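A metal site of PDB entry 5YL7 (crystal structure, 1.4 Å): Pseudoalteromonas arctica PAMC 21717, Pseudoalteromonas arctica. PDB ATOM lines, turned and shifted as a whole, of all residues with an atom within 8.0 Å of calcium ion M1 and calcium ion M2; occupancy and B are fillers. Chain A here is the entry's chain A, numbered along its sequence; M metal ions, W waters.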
ATOM      1  N   TYR A  58     -25.578 -20.611 -16.172  1.00  0.00           N
ATOM      2  CA  TYR A  58     -24.974 -21.721 -16.891  1.00  0.00           C
ATOM      3  C   TYR A  58     -25.871 -22.920 -16.878  1.00  0.00           C
ATOM      4  O   TYR A  58     -26.689 -23.084 -15.931  1.00  0.00           O
ATOM      5  CB  TYR A  58     -23.610 -22.134 -16.268  1.00  0.00           C
ATOM      6  CG  TYR A  58     -22.634 -22.629 -17.361  1.00  0.00           C
ATOM      7  CD1 TYR A  58     -21.968 -21.737 -18.131  1.00  0.00           C
ATOM      8  CD2 TYR A  58     -22.511 -23.974 -17.710  1.00  0.00           C
ATOM      9  CE1 TYR A  58     -21.189 -22.096 -19.197  1.00  0.00           C
ATOM     10  CE2 TYR A  58     -21.669 -24.327 -18.811  1.00  0.00           C
ATOM     11  CZ  TYR A  58     -21.123 -23.304 -19.489  1.00  0.00           C
ATOM     12  OH  TYR A  58     -20.311 -23.711 -20.610  1.00  0.00           O
ATOM     13  N   ASP A  59     -25.823 -23.746 -17.906  1.00  0.00           N
ATOM     14  CA  ASP A  59     -26.605 -24.930 -18.086  1.00  0.00           C
ATOM     15  C   ASP A  59     -25.704 -26.124 -17.959  1.00  0.00           C
ATOM     16  O   ASP A  59     -24.836 -26.393 -18.813  1.00  0.00           O
ATOM     17  CB  ASP A  59     -27.322 -24.861 -19.447  1.00  0.00           C
ATOM     18  CG  ASP A  59     -28.252 -25.983 -19.668  1.00  0.00           C
ATOM     19  OD1 ASP A  59     -28.186 -27.078 -19.124  1.00  0.00           O
ATOM     20  OD2 ASP A  59     -29.161 -25.780 -20.587  1.00  0.00           O
ATOM     21  N   MET A  60     -25.828 -26.848 -16.836  1.00  0.00           N
ATOM     22  CA  MET A  60     -25.009 -27.961 -16.490  1.00  0.00           C
ATOM     23  C   MET A  60     -25.464 -29.241 -16.987  1.00  0.00           C
ATOM     24  O   MET A  60     -24.857 -30.331 -16.711  1.00  0.00           O
ATOM     25  CB  MET A  60     -24.909 -28.076 -14.971  1.00  0.00           C
ATOM     26  CG  MET A  60     -24.266 -26.919 -14.308  1.00  0.00           C
ATOM     27  SD  MET A  60     -22.423 -26.911 -14.838  1.00  0.00           S
ATOM     28  CE  MET A  60     -21.972 -25.352 -13.987  1.00  0.00           C
ATOM     29  N   ILE A  61     -26.576 -29.335 -17.709  1.00  0.00           N
ATOM     30  CA  ILE A  61     -27.140 -30.616 -18.111  1.00  0.00           C
ATOM     31  C   ILE A  61     -26.299 -31.262 -19.245  1.00  0.00           C
ATOM     32  O   ILE A  61     -26.133 -30.700 -20.328  1.00  0.00           O
ATOM     33  CB  ILE A  61     -28.600 -30.545 -18.517  1.00  0.00           C
ATOM     34  CG1 ILE A  61     -29.430 -29.942 -17.430  1.00  0.00           C
ATOM     35  CG2 ILE A  61     -29.065 -31.957 -18.882  1.00  0.00           C
ATOM     36  CD1 ILE A  61     -30.846 -29.687 -17.857  1.00  0.00           C
ATOM     37  N   SER A  62     -25.700 -32.405 -18.887  1.00  0.00           N
ATOM     38  CA  SER A  62     -24.774 -33.111 -19.841  1.00  0.00           C
ATOM     39  C   SER A  62     -25.519 -34.055 -20.774  1.00  0.00           C
ATOM     40  O   SER A  62     -25.079 -34.201 -21.952  1.00  0.00           O
ATOM     41  CB  SER A  62     -23.714 -33.901 -19.008  1.00  0.00           C
ATOM     42  OG  SER A  62     -23.040 -33.142 -18.086  1.00  0.00           O
ATOM     43  N   ASN A  63     -26.594 -34.672 -20.364  1.00  0.00           N
ATOM     44  CA  ASN A  63     -27.323 -35.636 -21.208  1.00  0.00           C
ATOM     45  C   ASN A  63     -28.205 -34.917 -22.202  1.00  0.00           C
ATOM     46  O   ASN A  63     -29.048 -34.075 -21.769  1.00  0.00           O
ATOM     47  CB  ASN A  63     -28.068 -36.563 -20.275  1.00  0.00           C
ATOM     48  CG  ASN A  63     -28.966 -37.563 -20.982  1.00  0.00           C
ATOM     49  OD1 ASN A  63     -29.830 -37.256 -21.782  1.00  0.00           O
ATOM     50  ND2 ASN A  63     -28.869 -38.794 -20.537  1.00  0.00           N
ATOM     51  N   LEU A  64     -28.023 -35.113 -23.484  1.00  0.00           N
ATOM     52  CA  LEU A  64     -28.709 -34.350 -24.480  1.00  0.00           C
ATOM     53  C   LEU A  64     -30.204 -34.574 -24.415  1.00  0.00           C
ATOM     54  O   LEU A  64     -30.941 -33.618 -24.698  1.00  0.00           O
ATOM     55  CB  LEU A  64     -28.170 -34.732 -25.909  1.00  0.00           C
ATOM     56  CG  LEU A  64     -27.067 -33.711 -26.319  1.00  0.00           C
ATOM     57  CD1 LEU A  64     -25.789 -33.815 -25.514  1.00  0.00           C
ATOM     58  CD2 LEU A  64     -26.756 -33.838 -27.806  1.00  0.00           C
ATOM     59  N   VAL A  66     -32.083 -35.176 -21.776  1.00  0.00           N
ATOM     60  CA  VAL A  66     -32.572 -34.453 -20.619  1.00  0.00           C
ATOM     61  C   VAL A  66     -32.505 -32.961 -20.976  1.00  0.00           C
ATOM     62  O   VAL A  66     -33.457 -32.179 -20.690  1.00  0.00           O
ATOM     63  CB  VAL A  66     -31.748 -34.743 -19.384  1.00  0.00           C
ATOM     64  CG1 VAL A  66     -32.192 -33.931 -18.221  1.00  0.00           C
ATOM     65  CG2 VAL A  66     -31.866 -36.246 -19.011  1.00  0.00           C
ATOM     66  N   ALA A  67     -31.428 -32.513 -21.572  1.00  0.00           N
ATOM     67  CA  ALA A  67     -31.184 -31.109 -21.809  1.00  0.00           C
ATOM     68  C   ALA A  67     -32.236 -30.509 -22.741  1.00  0.00           C
ATOM     69  O   ALA A  67     -32.659 -29.359 -22.550  1.00  0.00           O
ATOM     70  CB  ALA A  67     -29.841 -30.896 -22.453  1.00  0.00           C
ATOM     71  N   ASN A  68     -32.644 -31.192 -23.817  1.00  0.00           N
ATOM     72  CA  ASN A  68     -33.713 -30.779 -24.675  1.00  0.00           C
ATOM     73  C   ASN A  68     -33.398 -29.440 -25.261  1.00  0.00           C
ATOM     74  O   ASN A  68     -34.344 -28.668 -25.503  1.00  0.00           O
ATOM     75  CB  ASN A  68     -35.062 -30.752 -23.926  1.00  0.00           C
ATOM     76  CG  ASN A  68     -36.259 -30.540 -24.821  1.00  0.00           C
ATOM     77  OD1 ASN A  68     -36.274 -31.034 -25.967  1.00  0.00           O
ATOM     78  ND2 ASN A  68     -37.241 -29.785 -24.379  1.00  0.00           N
ATOM     79  N   ASP A  69     -32.158 -29.132 -25.594  1.00  0.00           N
ATOM     80  CA  ASP A  69     -31.755 -27.851 -26.163  1.00  0.00           C
ATOM     81  C   ASP A  69     -30.695 -27.985 -27.249  1.00  0.00           C
ATOM     82  O   ASP A  69     -30.164 -26.998 -27.680  1.00  0.00           O
ATOM     83  CB  ASP A  69     -31.280 -26.907 -25.045  1.00  0.00           C
ATOM     84  CG  ASP A  69     -30.007 -27.338 -24.399  1.00  0.00           C
ATOM     85  OD1 ASP A  69     -29.457 -28.409 -24.792  1.00  0.00           O
ATOM     86  OD2 ASP A  69     -29.454 -26.550 -23.542  1.00  0.00           O
ATOM     87  N   GLY A  70     -30.433 -29.204 -27.672  1.00  0.00           N
ATOM     88  CA  GLY A  70     -29.566 -29.421 -28.843  1.00  0.00           C
ATOM     89  C   GLY A  70     -28.159 -29.771 -28.481  1.00  0.00           C
ATOM     90  O   GLY A  70     -27.361 -30.134 -29.415  1.00  0.00           O
ATOM     91  N   GLY A  71     -27.712 -29.812 -27.224  1.00  0.00           N
ATOM     92  CA  GLY A  71     -26.363 -30.120 -26.869  1.00  0.00           C
ATOM     93  C   GLY A  71     -26.196 -30.237 -25.398  1.00  0.00           C
ATOM     94  O   GLY A  71     -27.143 -30.099 -24.577  1.00  0.00           O
ATOM     95  N   GLY A  72     -24.998 -30.563 -25.025  1.00  0.00           N
ATOM     96  CA  GLY A  72     -24.562 -30.677 -23.617  1.00  0.00           C
ATOM     97  C   GLY A  72     -24.409 -29.404 -22.917  1.00  0.00           C
ATOM     98  O   GLY A  72     -25.135 -28.409 -23.173  1.00  0.00           O
ATOM     99  N   ARG A  73     -23.476 -29.304 -22.013  1.00  0.00           N
ATOM    100  CA  ARG A  73     -23.320 -28.119 -21.184  1.00  0.00           C
ATOM    101  C   ARG A  73     -23.188 -26.900 -22.022  1.00  0.00           C
ATOM    102  O   ARG A  73     -22.455 -26.876 -23.025  1.00  0.00           O
ATOM    103  CB  ARG A  73     -22.234 -28.315 -20.091  1.00  0.00           C
ATOM    104  CG  ARG A  73     -22.576 -29.433 -19.130  1.00  0.00           C
ATOM    105  CD  ARG A  73     -21.522 -29.456 -17.994  1.00  0.00           C
ATOM    106  NE  ARG A  73     -21.954 -30.365 -16.958  1.00  0.00           N
ATOM    107  CZ  ARG A  73     -21.208 -30.706 -15.898  1.00  0.00           C
ATOM    108  NH1 ARG A  73     -19.985 -30.216 -15.780  1.00  0.00           N
ATOM    109  NH2 ARG A  73     -21.769 -31.433 -15.005  1.00  0.00           N
ATOM    110  N   ASP A  74     -23.757 -25.797 -21.585  1.00  0.00           N
ATOM    111  CA  ASP A  74     -23.740 -24.584 -22.370  1.00  0.00           C
ATOM    112  C   ASP A  74     -24.054 -23.375 -21.557  1.00  0.00           C
ATOM    113  O   ASP A  74     -24.588 -23.505 -20.425  1.00  0.00           O
ATOM    114  CB  ASP A  74     -24.726 -24.658 -23.536  1.00  0.00           C
ATOM    115  CG  ASP A  74     -26.186 -24.658 -23.102  1.00  0.00           C
ATOM    116  OD1 ASP A  74     -26.733 -23.520 -22.982  1.00  0.00           O
ATOM    117  OD2 ASP A  74     -26.804 -25.685 -22.875  1.00  0.00           O
ATOM    118  N   SER A  75     -23.830 -22.169 -22.027  1.00  0.00           N
ATOM    119  CA  SER A  75     -23.977 -20.968 -21.245  1.00  0.00           C
ATOM    120  C   SER A  75     -25.423 -20.432 -21.137  1.00  0.00           C
ATOM    121  O   SER A  75     -25.577 -19.483 -20.392  1.00  0.00           O
ATOM    122  CB  SER A  75     -23.022 -19.849 -21.661  1.00  0.00           C
ATOM    123  OG  SER A  75     -23.438 -19.424 -22.921  1.00  0.00           O
ATOM    124  N   ASP A  76     -26.375 -21.034 -21.831  1.00  0.00           N
ATOM    125  CA  ASP A  76     -27.756 -20.473 -21.817  1.00  0.00           C
ATOM    126  C   ASP A  76     -28.597 -21.363 -20.905  1.00  0.00           C
ATOM    127  O   ASP A  76     -28.962 -22.478 -21.221  1.00  0.00           O
ATOM    128  CB  ASP A  76     -28.272 -20.484 -23.238  1.00  0.00           C
ATOM    129  CG  ASP A  76     -29.591 -19.865 -23.353  1.00  0.00           C
ATOM    130  OD1 ASP A  76     -30.249 -19.528 -22.354  1.00  0.00           O
ATOM    131  OD2 ASP A  76     -30.041 -19.543 -24.499  1.00  0.00           O
ATOM    132  N   ALA A  77     -28.950 -20.801 -19.743  1.00  0.00           N
ATOM    133  CA  ALA A  77     -29.710 -21.500 -18.707  1.00  0.00           C
ATOM    134  C   ALA A  77     -31.176 -21.329 -18.876  1.00  0.00           C
ATOM    135  O   ALA A  77     -31.982 -21.607 -17.975  1.00  0.00           O
ATOM    136  CB  ALA A  77     -29.269 -20.994 -17.331  1.00  0.00           C
ATOM    137  N   ARG A  78     -31.674 -20.828 -20.040  1.00  0.00           N
ATOM    138  CA  ARG A  78     -33.090 -20.816 -20.259  1.00  0.00           C
ATOM    139  C   ARG A  78     -33.693 -22.185 -20.283  1.00  0.00           C
ATOM    140  O   ARG A  78     -33.056 -23.172 -20.659  1.00  0.00           O
ATOM    141  CB  ARG A  78     -33.445 -20.013 -21.512  1.00  0.00           C
ATOM    142  CG  ARG A  78     -33.279 -18.547 -21.320  1.00  0.00           C
ATOM    143  CD  ARG A  78     -33.548 -17.722 -22.554  1.00  0.00           C
ATOM    144  NE  ARG A  78     -33.304 -16.319 -22.326  1.00  0.00           N
ATOM    145  CZ  ARG A  78     -33.778 -15.297 -23.079  1.00  0.00           C
ATOM    146  NH1 ARG A  78     -34.569 -15.534 -24.074  1.00  0.00           N
ATOM    147  NH2 ARG A  78     -33.452 -14.077 -22.750  1.00  0.00           N
ATOM    148  N   ASP A  79     -34.973 -22.284 -19.872  1.00  0.00           N
ATOM    149  CA  ASP A  79     -35.684 -23.529 -19.813  1.00  0.00           C
ATOM    150  C   ASP A  79     -36.363 -23.774 -21.147  1.00  0.00           C
ATOM    151  O   ASP A  79     -37.288 -23.016 -21.490  1.00  0.00           O
ATOM    152  CB  ASP A  79     -36.728 -23.447 -18.703  1.00  0.00           C
ATOM    153  CG  ASP A  79     -37.420 -24.704 -18.372  1.00  0.00           C
ATOM    154  OD1 ASP A  79     -37.296 -25.708 -19.126  1.00  0.00           O
ATOM    155  OD2 ASP A  79     -38.186 -24.715 -17.359  1.00  0.00           O
ATOM    156  N   PRO A  80     -36.001 -24.821 -21.883  1.00  0.00           N
ATOM    157  CA  PRO A  80     -36.704 -25.139 -23.157  1.00  0.00           C
ATOM    158  C   PRO A  80     -38.014 -25.770 -22.947  1.00  0.00           C
ATOM    159  O   PRO A  80     -38.747 -25.987 -23.946  1.00  0.00           O
ATOM    160  CB  PRO A  80     -35.729 -26.048 -23.835  1.00  0.00           C
ATOM    161  CG  PRO A  80     -35.068 -26.855 -22.695  1.00  0.00           C
ATOM    162  CD  PRO A  80     -34.966 -25.798 -21.594  1.00  0.00           C
ATOM    163  N   ARG A 131     -29.031 -24.091 -14.605  1.00  0.00           N
ATOM    164  CA  ARG A 131     -29.927 -25.077 -15.118  1.00  0.00           C
ATOM    165  C   ARG A 131     -29.350 -26.462 -14.887  1.00  0.00           C
ATOM    166  O   ARG A 131     -28.320 -26.800 -15.478  1.00  0.00           O
ATOM    167  CB  ARG A 131     -30.337 -24.837 -16.587  1.00  0.00           C
ATOM    168  CG  ARG A 131     -31.208 -25.896 -17.129  1.00  0.00           C
ATOM    169  CD  ARG A 131     -31.858 -25.454 -18.433  1.00  0.00           C
ATOM    170  NE  ARG A 131     -32.774 -26.485 -18.862  1.00  0.00           N
ATOM    171  CZ  ARG A 131     -32.649 -27.374 -19.853  1.00  0.00           C
ATOM    172  NH1 ARG A 131     -31.611 -27.337 -20.643  1.00  0.00           N
ATOM    173  NH2 ARG A 131     -33.553 -28.304 -20.025  1.00  0.00           N
HETATM  174 CA    CA M   1     -29.016 -24.478 -22.556  1.00  0.00          CA
HETATM  175 CA    CA M   2     -27.347 -27.880 -23.601  1.00  0.00          CA
HETATM  176  O   HOH W   1     -27.638 -28.644 -21.401  1.00  0.00           O
HETATM  177  O   HOH W   2     -29.159 -23.714 -24.783  1.00  0.00           O
HETATM  178  O   HOH W   3     -26.552 -27.149 -25.682  1.00  0.00           O
HETATM  179  O   HOH W   4     -31.317 -23.987 -22.590  1.00  0.00           O
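OD1 of Asp 76 is in hydrogen-bond range of N of Arg 78, at 3.0 Å. The guanidinium group (NH1) of Arg 131 sits close to the side-chain carboxylate (OD2) of Asp 69, at 3.7 Å. The guanidinium group of Arg 131 is in salt-bridge range of the side-chain carboxylate of Asp 59 (3.8 Å). The side-chain carboxylate (OD1) of Asp 59 is in hydrogen-bond range of the backbone NH (N) of Ile 61, at 3.1 Å.
Four residues have an atom within 4 Å of calcium ion M1: Asp 59, Asp 69, Asp 74 and Asp 76.
Four residues have an atom within 4 Å of calcium ion M2: Asp 69, Gly 71, Gly 72 and Asp 74.
Calcium ion M1 is bound by the side-chain carboxylate (OD2) of Asp 69 (2.3 Å), water W4 (2.4 Å), water W2 (2.4 Å), the side-chain carboxylate (OD2) of Asp 59 (2.4 Å), the backbone carbonyl oxygen (O) of Asp 76 (2.4 Å), the side-chain carboxylate (OD1) of Asp 74 (2.5 Å) and the side-chain carboxylate (OD2) of Asp 74 (2.5 Å). Calcium ion M1 has seven donor atoms within binding distance.
Calcium ion M2 is bound by O of Gly 72 (2.3 Å), water W3 (2.3 Å), water W1 (2.3 Å), OD2 of Asp 74 (2.4 Å), O of Gly 71 (2.4 Å), OD1 of Asp 69 (2.5 Å) and OD2 of Asp 69 (2.5 Å). Calcium ion M2 has seven donor atoms within binding distance.
Water W1 bridges the backbone carbonyl oxygen (O) of Ile 61 and the side-chain carboxylate (OD1) of Asp 59.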
